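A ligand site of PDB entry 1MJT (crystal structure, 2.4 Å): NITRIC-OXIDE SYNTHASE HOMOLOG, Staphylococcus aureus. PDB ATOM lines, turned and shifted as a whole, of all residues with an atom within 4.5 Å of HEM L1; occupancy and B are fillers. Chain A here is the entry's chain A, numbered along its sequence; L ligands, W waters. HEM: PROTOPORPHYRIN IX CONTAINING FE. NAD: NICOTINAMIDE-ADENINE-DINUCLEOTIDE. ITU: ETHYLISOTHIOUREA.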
ATOM      1  N   TRP A  57       5.558  16.946   2.582  1.00  0.00           N
ATOM      2  CA  TRP A  57       5.394  18.389   2.430  1.00  0.00           C
ATOM      3  C   TRP A  57       5.141  18.961   3.832  1.00  0.00           C
ATOM      4  O   TRP A  57       5.719  19.975   4.215  1.00  0.00           O
ATOM      5  CB  TRP A  57       4.192  18.671   1.504  1.00  0.00           C
ATOM      6  CG  TRP A  57       3.836  20.149   1.293  1.00  0.00           C
ATOM      7  CD1 TRP A  57       4.474  21.242   1.832  1.00  0.00           C
ATOM      8  CD2 TRP A  57       2.746  20.674   0.522  1.00  0.00           C
ATOM      9  NE1 TRP A  57       3.840  22.407   1.439  1.00  0.00           N
ATOM     10  CE2 TRP A  57       2.778  22.088   0.627  1.00  0.00           C
ATOM     11  CE3 TRP A  57       1.736  20.085  -0.275  1.00  0.00           C
ATOM     12  CZ2 TRP A  57       1.840  22.921  -0.012  1.00  0.00           C
ATOM     13  CZ3 TRP A  57       0.806  20.923  -0.912  1.00  0.00           C
ATOM     14  CH2 TRP A  57       0.865  22.332  -0.768  1.00  0.00           C
ATOM     15  N   SER A  60       8.204  19.476   5.729  1.00  0.00           N
ATOM     16  CA  SER A  60       9.162  20.369   5.076  1.00  0.00           C
ATOM     17  C   SER A  60       9.386  21.646   5.862  1.00  0.00           C
ATOM     18  O   SER A  60       8.768  22.675   5.588  1.00  0.00           O
ATOM     19  CB  SER A  60       8.684  20.708   3.658  1.00  0.00           C
ATOM     20  OG  SER A  60       8.915  19.599   2.792  1.00  0.00           O
ATOM     21  N   ARG A  62      11.448  24.074   5.891  1.00  0.00           N
ATOM     22  CA  ARG A  62      11.717  25.345   5.220  1.00  0.00           C
ATOM     23  C   ARG A  62      10.551  25.884   4.395  1.00  0.00           C
ATOM     24  O   ARG A  62      10.690  26.891   3.705  1.00  0.00           O
ATOM     25  CB  ARG A  62      12.943  25.188   4.326  1.00  0.00           C
ATOM     26  CG  ARG A  62      14.040  24.287   4.891  1.00  0.00           C
ATOM     27  CD  ARG A  62      15.370  24.548   4.199  1.00  0.00           C
ATOM     28  NE  ARG A  62      16.229  23.370   4.175  1.00  0.00           N
ATOM     29  CZ  ARG A  62      15.971  22.274   3.467  1.00  0.00           C
ATOM     30  NH1 ARG A  62      14.868  22.215   2.729  1.00  0.00           N
ATOM     31  NH2 ARG A  62      16.800  21.244   3.499  1.00  0.00           N
ATOM     32  N   CYS A  63       9.407  25.223   4.480  1.00  0.00           N
ATOM     33  CA  CYS A  63       8.222  25.617   3.713  1.00  0.00           C
ATOM     34  C   CYS A  63       7.201  26.459   4.500  1.00  0.00           C
ATOM     35  O   CYS A  63       6.588  25.973   5.443  1.00  0.00           O
ATOM     36  CB  CYS A  63       7.539  24.364   3.154  1.00  0.00           C
ATOM     37  SG  CYS A  63       5.999  24.730   2.312  1.00  0.00           S
ATOM     38  N   ILE A  64       7.019  27.703   4.087  1.00  0.00           N
ATOM     39  CA  ILE A  64       6.075  28.601   4.757  1.00  0.00           C
ATOM     40  C   ILE A  64       4.625  28.367   4.328  1.00  0.00           C
ATOM     41  O   ILE A  64       3.682  28.801   5.000  1.00  0.00           O
ATOM     42  CB  ILE A  64       6.442  30.081   4.487  1.00  0.00           C
ATOM     43  CG1 ILE A  64       5.695  30.986   5.461  1.00  0.00           C
ATOM     44  CG2 ILE A  64       6.074  30.452   3.045  1.00  0.00           C
ATOM     45  CD1 ILE A  64       6.106  30.779   6.886  1.00  0.00           C
ATOM     46  N   GLY A  65       4.449  27.655   3.207  1.00  0.00           N
ATOM     47  CA  GLY A  65       3.117  27.411   2.690  1.00  0.00           C
ATOM     48  C   GLY A  65       2.490  26.066   3.009  1.00  0.00           C
ATOM     49  O   GLY A  65       1.624  25.590   2.272  1.00  0.00           O
ATOM     50  N   PHE A  68      -1.551  24.391   3.040  1.00  0.00           N
ATOM     51  CA  PHE A  68      -2.256  23.659   1.999  1.00  0.00           C
ATOM     52  C   PHE A  68      -1.737  22.247   1.739  1.00  0.00           C
ATOM     53  O   PHE A  68      -2.048  21.664   0.697  1.00  0.00           O
ATOM     54  CB  PHE A  68      -2.194  24.445   0.678  1.00  0.00           C
ATOM     55  CG  PHE A  68      -2.328  25.945   0.849  1.00  0.00           C
ATOM     56  CD1 PHE A  68      -1.245  26.717   1.244  1.00  0.00           C
ATOM     57  CD2 PHE A  68      -3.540  26.577   0.598  1.00  0.00           C
ATOM     58  CE1 PHE A  68      -1.365  28.095   1.400  1.00  0.00           C
ATOM     59  CE2 PHE A  68      -3.671  27.959   0.747  1.00  0.00           C
ATOM     60  CZ  PHE A  68      -2.582  28.714   1.151  1.00  0.00           C
ATOM     61  N   LEU A  72      -2.452  18.657  -1.850  1.00  0.00           N
ATOM     62  CA  LEU A  72      -1.595  18.103  -2.899  1.00  0.00           C
ATOM     63  C   LEU A  72      -2.288  17.115  -3.822  1.00  0.00           C
ATOM     64  O   LEU A  72      -3.065  16.265  -3.393  1.00  0.00           O
ATOM     65  CB  LEU A  72      -0.376  17.447  -2.255  1.00  0.00           C
ATOM     66  CG  LEU A  72       0.807  17.048  -3.143  1.00  0.00           C
ATOM     67  CD1 LEU A  72       1.313  18.250  -3.907  1.00  0.00           C
ATOM     68  CD2 LEU A  72       1.916  16.492  -2.260  1.00  0.00           C
ATOM     69  N   PRO A 105      -1.344  22.436  -6.481  1.00  0.00           N
ATOM     70  CA  PRO A 105      -0.218  21.665  -5.941  1.00  0.00           C
ATOM     71  C   PRO A 105      -0.159  20.296  -6.594  1.00  0.00           C
ATOM     72  O   PRO A 105      -1.096  19.511  -6.450  1.00  0.00           O
ATOM     73  CB  PRO A 105      -0.557  21.543  -4.452  1.00  0.00           C
ATOM     74  CG  PRO A 105      -1.375  22.742  -4.183  1.00  0.00           C
ATOM     75  CD  PRO A 105      -2.265  22.834  -5.405  1.00  0.00           C
ATOM     76  N   ILE A 206      10.019  22.184  -8.422  1.00  0.00           N
ATOM     77  CA  ILE A 206      11.305  21.675  -7.987  1.00  0.00           C
ATOM     78  C   ILE A 206      11.487  20.258  -8.529  1.00  0.00           C
ATOM     79  O   ILE A 206      10.633  19.401  -8.333  1.00  0.00           O
ATOM     80  CB  ILE A 206      11.415  21.640  -6.452  1.00  0.00           C
ATOM     81  CG1 ILE A 206      11.268  23.047  -5.889  1.00  0.00           C
ATOM     82  CG2 ILE A 206      12.790  21.095  -6.042  1.00  0.00           C
ATOM     83  CD1 ILE A 206      11.460  23.115  -4.379  1.00  0.00           C
ATOM     84  N   MET A 209      15.243  17.263  -5.946  1.00  0.00           N
ATOM     85  CA  MET A 209      15.265  16.802  -4.567  1.00  0.00           C
ATOM     86  C   MET A 209      14.824  15.354  -4.460  1.00  0.00           C
ATOM     87  O   MET A 209      14.212  14.814  -5.386  1.00  0.00           O
ATOM     88  CB  MET A 209      14.339  17.663  -3.704  1.00  0.00           C
ATOM     89  CG  MET A 209      14.794  19.103  -3.582  1.00  0.00           C
ATOM     90  SD  MET A 209      13.921  19.980  -2.280  1.00  0.00           S
ATOM     91  CE  MET A 209      14.785  19.357  -0.816  1.00  0.00           C
ATOM     92  N   PHE A 223       7.701  18.441  -7.922  1.00  0.00           N
ATOM     93  CA  PHE A 223       6.507  18.933  -7.242  1.00  0.00           C
ATOM     94  C   PHE A 223       6.408  20.444  -7.382  1.00  0.00           C
ATOM     95  O   PHE A 223       7.405  21.109  -7.645  1.00  0.00           O
ATOM     96  CB  PHE A 223       6.559  18.571  -5.763  1.00  0.00           C
ATOM     97  CG  PHE A 223       7.816  19.003  -5.050  1.00  0.00           C
ATOM     98  CD1 PHE A 223       8.954  18.186  -5.057  1.00  0.00           C
ATOM     99  CD2 PHE A 223       7.864  20.200  -4.350  1.00  0.00           C
ATOM    100  CE1 PHE A 223      10.098  18.552  -4.358  1.00  0.00           C
ATOM    101  CE2 PHE A 223       9.008  20.583  -3.644  1.00  0.00           C
ATOM    102  CZ  PHE A 223      10.129  19.756  -3.656  1.00  0.00           C
ATOM    103  N   ASN A 224       5.202  20.994  -7.211  1.00  0.00           N
ATOM    104  CA  ASN A 224       5.024  22.439  -7.324  1.00  0.00           C
ATOM    105  C   ASN A 224       3.939  23.043  -6.439  1.00  0.00           C
ATOM    106  O   ASN A 224       3.061  22.357  -5.913  1.00  0.00           O
ATOM    107  CB  ASN A 224       4.727  22.836  -8.773  1.00  0.00           C
ATOM    108  CG  ASN A 224       3.293  22.522  -9.182  1.00  0.00           C
ATOM    109  OD1 ASN A 224       2.950  21.384  -9.480  1.00  0.00           O
ATOM    110  ND2 ASN A 224       2.441  23.544  -9.165  1.00  0.00           N
ATOM    111  N   GLY A 225       4.037  24.356  -6.281  1.00  0.00           N
ATOM    112  CA  GLY A 225       3.082  25.139  -5.524  1.00  0.00           C
ATOM    113  C   GLY A 225       2.977  26.429  -6.329  1.00  0.00           C
ATOM    114  O   GLY A 225       3.067  26.402  -7.561  1.00  0.00           O
ATOM    115  N   TRP A 226       2.784  27.561  -5.659  1.00  0.00           N
ATOM    116  CA  TRP A 226       2.719  28.832  -6.369  1.00  0.00           C
ATOM    117  C   TRP A 226       3.698  29.744  -5.640  1.00  0.00           C
ATOM    118  O   TRP A 226       4.052  29.495  -4.485  1.00  0.00           O
ATOM    119  CB  TRP A 226       1.301  29.412  -6.371  1.00  0.00           C
ATOM    120  CG  TRP A 226       0.647  29.466  -5.034  1.00  0.00           C
ATOM    121  CD1 TRP A 226       0.869  30.375  -4.032  1.00  0.00           C
ATOM    122  CD2 TRP A 226      -0.318  28.544  -4.526  1.00  0.00           C
ATOM    123  NE1 TRP A 226       0.105  30.064  -2.927  1.00  0.00           N
ATOM    124  CE2 TRP A 226      -0.635  28.941  -3.207  1.00  0.00           C
ATOM    125  CE3 TRP A 226      -0.954  27.406  -5.062  1.00  0.00           C
ATOM    126  CZ2 TRP A 226      -1.561  28.251  -2.415  1.00  0.00           C
ATOM    127  CZ3 TRP A 226      -1.860  26.716  -4.259  1.00  0.00           C
ATOM    128  CH2 TRP A 226      -2.158  27.150  -2.954  1.00  0.00           C
ATOM    129  N   MET A 228       5.611  33.095  -3.860  1.00  0.00           N
ATOM    130  CA  MET A 228       5.413  34.030  -2.751  1.00  0.00           C
ATOM    131  C   MET A 228       6.322  35.172  -3.250  1.00  0.00           C
ATOM    132  O   MET A 228       7.510  34.953  -3.507  1.00  0.00           O
ATOM    133  CB  MET A 228       5.923  33.391  -1.457  1.00  0.00           C
ATOM    134  CG  MET A 228       5.644  34.176  -0.203  1.00  0.00           C
ATOM    135  SD  MET A 228       6.897  35.396   0.093  1.00  0.00           S
ATOM    136  CE  MET A 228       8.123  34.377   0.909  1.00  0.00           C
ATOM    137  N   GLU A 231      10.290  35.642  -3.482  1.00  0.00           N
ATOM    138  CA  GLU A 231      11.102  34.654  -4.178  1.00  0.00           C
ATOM    139  C   GLU A 231      11.569  35.250  -5.494  1.00  0.00           C
ATOM    140  O   GLU A 231      12.732  35.124  -5.873  1.00  0.00           O
ATOM    141  CB  GLU A 231      10.303  33.379  -4.452  1.00  0.00           C
ATOM    142  CG  GLU A 231       9.828  32.681  -3.190  1.00  0.00           C
ATOM    143  CD  GLU A 231       9.215  31.342  -3.480  1.00  0.00           C
ATOM    144  OE1 GLU A 231       9.974  30.408  -3.813  1.00  0.00           O
ATOM    145  OE2 GLU A 231       7.955  31.228  -3.376  1.00  0.00           O
ATOM    146  N   ARG A 235      14.975  37.717  -4.254  1.00  0.00           N
ATOM    147  CA  ARG A 235      16.041  36.783  -4.574  1.00  0.00           C
ATOM    148  C   ARG A 235      16.304  36.599  -6.065  1.00  0.00           C
ATOM    149  O   ARG A 235      17.415  36.857  -6.518  1.00  0.00           O
ATOM    150  CB  ARG A 235      15.719  35.430  -3.927  1.00  0.00           C
ATOM    151  CG  ARG A 235      15.316  35.529  -2.444  1.00  0.00           C
ATOM    152  CD  ARG A 235      16.400  36.180  -1.583  1.00  0.00           C
ATOM    153  NE  ARG A 235      17.631  35.411  -1.593  1.00  0.00           N
ATOM    154  CZ  ARG A 235      17.761  34.193  -1.065  1.00  0.00           C
ATOM    155  NH1 ARG A 235      16.711  33.614  -0.495  1.00  0.00           N
ATOM    156  NH2 ARG A 235      18.915  33.556  -1.107  1.00  0.00           N
ATOM    157  N   VAL A 288       1.112  34.851  -3.656  1.00  0.00           N
ATOM    158  CA  VAL A 288       0.768  35.284  -2.316  1.00  0.00           C
ATOM    159  C   VAL A 288       1.879  36.195  -1.810  1.00  0.00           C
ATOM    160  O   VAL A 288       3.043  35.957  -2.108  1.00  0.00           O
ATOM    161  CB  VAL A 288       0.627  34.073  -1.368  1.00  0.00           C
ATOM    162  CG1 VAL A 288       1.924  33.285  -1.328  1.00  0.00           C
ATOM    163  CG2 VAL A 288       0.229  34.547   0.026  1.00  0.00           C
ATOM    164  N   TRP A 317      14.496  30.253   7.163  1.00  0.00           N
ATOM    165  CA  TRP A 317      13.800  30.120   5.885  1.00  0.00           C
ATOM    166  C   TRP A 317      12.363  30.637   5.940  1.00  0.00           C
ATOM    167  O   TRP A 317      11.911  31.348   5.047  1.00  0.00           O
ATOM    168  CB  TRP A 317      13.801  28.666   5.415  1.00  0.00           C
ATOM    169  CG  TRP A 317      15.095  28.231   4.767  1.00  0.00           C
ATOM    170  CD1 TRP A 317      16.310  28.104   5.375  1.00  0.00           C
ATOM    171  CD2 TRP A 317      15.283  27.838   3.395  1.00  0.00           C
ATOM    172  NE1 TRP A 317      17.242  27.654   4.470  1.00  0.00           N
ATOM    173  CE2 TRP A 317      16.643  27.484   3.252  1.00  0.00           C
ATOM    174  CE3 TRP A 317      14.431  27.739   2.284  1.00  0.00           C
ATOM    175  CZ2 TRP A 317      17.171  27.042   2.029  1.00  0.00           C
ATOM    176  CZ3 TRP A 317      14.970  27.294   1.067  1.00  0.00           C
ATOM    177  CH2 TRP A 317      16.326  26.952   0.953  1.00  0.00           C
ATOM    178  N   PHE A 343      11.508  15.713   2.106  1.00  0.00           N
ATOM    179  CA  PHE A 343      12.229  16.026   0.875  1.00  0.00           C
ATOM    180  C   PHE A 343      13.671  16.370   1.244  1.00  0.00           C
ATOM    181  O   PHE A 343      13.907  17.164   2.149  1.00  0.00           O
ATOM    182  CB  PHE A 343      11.576  17.208   0.179  1.00  0.00           C
ATOM    183  CG  PHE A 343      10.234  16.903  -0.383  1.00  0.00           C
ATOM    184  CD1 PHE A 343      10.113  16.192  -1.569  1.00  0.00           C
ATOM    185  CD2 PHE A 343       9.087  17.328   0.271  1.00  0.00           C
ATOM    186  CE1 PHE A 343       8.866  15.915  -2.104  1.00  0.00           C
ATOM    187  CE2 PHE A 343       7.823  17.051  -0.249  1.00  0.00           C
ATOM    188  CZ  PHE A 343       7.714  16.343  -1.441  1.00  0.00           C
ATOM    189  N   TYR A 345      17.927  17.086  -0.240  1.00  0.00           N
ATOM    190  CA  TYR A 345      18.747  17.486  -1.379  1.00  0.00           C
ATOM    191  C   TYR A 345      19.478  16.243  -1.852  1.00  0.00           C
ATOM    192  O   TYR A 345      19.635  15.292  -1.102  1.00  0.00           O
ATOM    193  CB  TYR A 345      19.768  18.542  -0.962  1.00  0.00           C
ATOM    194  CG  TYR A 345      19.172  19.841  -0.486  1.00  0.00           C
ATOM    195  CD1 TYR A 345      18.187  20.504  -1.235  1.00  0.00           C
ATOM    196  CD2 TYR A 345      19.618  20.444   0.698  1.00  0.00           C
ATOM    197  CE1 TYR A 345      17.666  21.723  -0.813  1.00  0.00           C
ATOM    198  CE2 TYR A 345      19.097  21.663   1.120  1.00  0.00           C
ATOM    199  CZ  TYR A 345      18.128  22.304   0.362  1.00  0.00           C
ATOM    200  OH  TYR A 345      17.631  23.521   0.785  1.00  0.00           O
HETATM  201  CHA HEM L   1      10.350  26.035   0.197  1.00  0.00           C
HETATM  202  CHB HEM L   1       6.252  28.558  -0.455  1.00  0.00           C
HETATM  203  CHC HEM L   1       4.108  24.527  -2.027  1.00  0.00           C
HETATM  204  CHD HEM L   1       7.925  21.920  -0.539  1.00  0.00           C
HETATM  205  C1A HEM L   1       9.443  27.063  -0.034  1.00  0.00           C
HETATM  206  C2A HEM L   1       9.795  28.491  -0.018  1.00  0.00           C
HETATM  207  C3A HEM L   1       8.638  29.190  -0.111  1.00  0.00           C
HETATM  208  C4A HEM L   1       7.577  28.212  -0.247  1.00  0.00           C
HETATM  209  CMA HEM L   1       8.515  30.717  -0.059  1.00  0.00           C
HETATM  210  CAA HEM L   1      11.168  29.133   0.075  1.00  0.00           C
HETATM  211  CBA HEM L   1      11.932  28.950  -1.226  1.00  0.00           C
HETATM  212  CGA HEM L   1      13.227  29.707  -1.242  1.00  0.00           C
HETATM  213  O1A HEM L   1      13.197  30.946  -1.079  1.00  0.00           O
HETATM  214  O2A HEM L   1      14.288  29.069  -1.400  1.00  0.00           O
HETATM  215  C1B HEM L   1       5.237  27.638  -0.725  1.00  0.00           C
HETATM  216  C2B HEM L   1       3.958  28.059  -1.246  1.00  0.00           C
HETATM  217  C3B HEM L   1       3.346  26.939  -1.741  1.00  0.00           C
HETATM  218  C4B HEM L   1       4.267  25.821  -1.509  1.00  0.00           C
HETATM  219  CMB HEM L   1       3.432  29.484  -1.283  1.00  0.00           C
HETATM  220  CAB HEM L   1       2.131  26.959  -2.420  1.00  0.00           C
HETATM  221  CBB HEM L   1       1.060  25.871  -2.365  1.00  0.00           C
HETATM  222  C1C HEM L   1       5.011  23.487  -1.839  1.00  0.00           C
HETATM  223  C2C HEM L   1       4.770  22.089  -2.215  1.00  0.00           C
HETATM  224  C3C HEM L   1       5.763  21.339  -1.667  1.00  0.00           C
HETATM  225  C4C HEM L   1       6.667  22.296  -1.047  1.00  0.00           C
HETATM  226  CMC HEM L   1       3.612  21.540  -3.028  1.00  0.00           C
HETATM  227  CAC HEM L   1       5.893  19.939  -1.522  1.00  0.00           C
HETATM  228  CBC HEM L   1       5.266  18.791  -2.294  1.00  0.00           C
HETATM  229  C1D HEM L   1       8.869  22.818  -0.089  1.00  0.00           C
HETATM  230  C2D HEM L   1      10.239  22.431   0.166  1.00  0.00           C
HETATM  231  C3D HEM L   1      10.930  23.573   0.381  1.00  0.00           C
HETATM  232  C4D HEM L   1       9.992  24.691   0.233  1.00  0.00           C
HETATM  233  CMD HEM L   1      10.806  21.030   0.146  1.00  0.00           C
HETATM  234  CAD HEM L   1      12.411  23.651   0.618  1.00  0.00           C
HETATM  235  CBD HEM L   1      13.144  23.508  -0.699  1.00  0.00           C
HETATM  236  CGD HEM L   1      14.596  23.885  -0.602  1.00  0.00           C
HETATM  237  O1D HEM L   1      15.299  23.303   0.249  1.00  0.00           O
HETATM  238  O2D HEM L   1      15.033  24.770  -1.372  1.00  0.00           O
HETATM  239  NA  HEM L   1       8.077  26.906  -0.190  1.00  0.00           N
HETATM  240  NB  HEM L   1       5.417  26.273  -0.833  1.00  0.00           N
HETATM  241  NC  HEM L   1       6.201  23.611  -1.113  1.00  0.00           N
HETATM  242  ND  HEM L   1       8.700  24.206  -0.017  1.00  0.00           N
HETATM  243 FE   HEM L   1       7.032  25.215  -0.263  1.00  0.00          FE
HETATM  244  PA  NAD L   2      22.181  26.606   9.096  1.00  0.00           P
HETATM  245  O1A NAD L   2      21.510  25.312   9.459  1.00  0.00           O
HETATM  246  O2A NAD L   2      22.053  27.104   7.688  1.00  0.00           O
HETATM  247  O5B NAD L   2      23.769  26.450   9.562  1.00  0.00           O
HETATM  248  O3  NAD L   2      21.697  27.858  10.048  1.00  0.00           O
HETATM  249  PN  NAD L   2      21.603  29.469   9.938  1.00  0.00           P
HETATM  250  O1N NAD L   2      20.609  30.002  10.891  1.00  0.00           O
HETATM  251  O2N NAD L   2      23.120  29.827  10.015  1.00  0.00           O
HETATM  252  O5D NAD L   2      21.008  29.561   8.433  1.00  0.00           O
HETATM  253  C5D NAD L   2      21.146  30.692   7.636  1.00  0.00           C
HETATM  254  C4D NAD L   2      21.387  30.201   6.239  1.00  0.00           C
HETATM  255  O4D NAD L   2      20.086  30.079   5.560  1.00  0.00           O
HETATM  256  C3D NAD L   2      22.247  31.168   5.387  1.00  0.00           C
HETATM  257  O3D NAD L   2      23.316  30.387   4.825  1.00  0.00           O
HETATM  258  C2D NAD L   2      21.252  31.755   4.355  1.00  0.00           C
HETATM  259  O2D NAD L   2      21.822  32.198   3.102  1.00  0.00           O
HETATM  260  C1D NAD L   2      20.230  30.655   4.206  1.00  0.00           C
HETATM  261  N1N NAD L   2      18.878  31.059   3.828  1.00  0.00           N
HETATM  262  C2N NAD L   2      18.539  30.636   2.514  1.00  0.00           C
HETATM  263  C3N NAD L   2      17.254  30.976   2.004  1.00  0.00           C
HETATM  264  C7N NAD L   2      16.749  30.572   0.579  1.00  0.00           C
HETATM  265  O7N NAD L   2      15.537  30.478   0.353  1.00  0.00           O
HETATM  266  N7N NAD L   2      17.667  30.332  -0.396  1.00  0.00           N
HETATM  267  C4N NAD L   2      16.278  31.747   2.777  1.00  0.00           C
HETATM  268  C5N NAD L   2      16.730  32.135   4.098  1.00  0.00           C
HETATM  269  C6N NAD L   2      17.966  31.844   4.674  1.00  0.00           C
HETATM  270  C1  ITU L   3       7.828  23.664  -5.136  1.00  0.00           C
HETATM  271  C2  ITU L   3       8.049  24.737  -4.161  1.00  0.00           C
HETATM  272  S   ITU L   3       6.790  26.016  -4.228  1.00  0.00           S
HETATM  273  C3  ITU L   3       7.542  27.615  -3.937  1.00  0.00           C
HETATM  274  N1  ITU L   3       8.840  27.707  -3.714  1.00  0.00           N
HETATM  275  N2  ITU L   3       6.790  28.704  -3.937  1.00  0.00           N
HETATM  276  O   HOH W   1      18.059  25.166  -1.889  1.00  0.00           O
HETATM  277  O   HOH W   2       9.459  29.294   2.939  1.00  0.00           O
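NH1 of Arg 62 lies within salt-bridge range of O1D of HEM L1, 2.7 Å away.
O7N of NAD L2 sits close to NH1 of Arg 235, 3.5 Å away.
The side-chain hydroxyl of Tyr 345 sits at hydrogen-bond distance from an oxygen (O1D) of HEM L1.
The backbone carbonyl oxygen (O) of Trp 226 is in hydrogen-bond range of a nitrogen (N2) of ITU L3, at 2.9 Å.
The side-chain carboxylate (OE2) of Glu 231 is in hydrogen-bond range of a nitrogen (N2) of ITU L3.
O2A of HEM L1 lies close to O7N of NAD L2.
SG of Cys 63 sits at hydrogen-bond distance from NE1 of Trp 57, at 3.3 Å.
OE2 of Glu 231 sits at hydrogen-bond distance from N of Met 228 (3.0 Å).
N of Ile 206 sits at hydrogen-bond distance from O of Phe 223 (2.9 Å).
SG of Cys 63 lies close to N of Gly 65, 3.4 Å away.
SG of Cys 63 lies close to NB of HEM L1, at 3.6 Å.
Merely in contact with HEM L1: Trp 57, Ser 60, Ile 64, Met 209, Phe 223, Asn 224, Gly 225, Trp 226, Met 228, Glu 231, Trp 317 and Phe 343.
Within 4 Å of HEM L1: Trp 57, Ser 60, Arg 62, Cys 63, Ile 64, Met 209, Phe 223, Asn 224, Gly 225, Trp 226, Met 228, Glu 231, Trp 317, Phe 343 and Tyr 345.
The nearest printed residue that does not touch HEM L1 is Gly 65 (4.01 Å).
Water W1 bridges O2D of HEM L1 (3.1 Å) and OH of Tyr 345 (3.2 Å).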
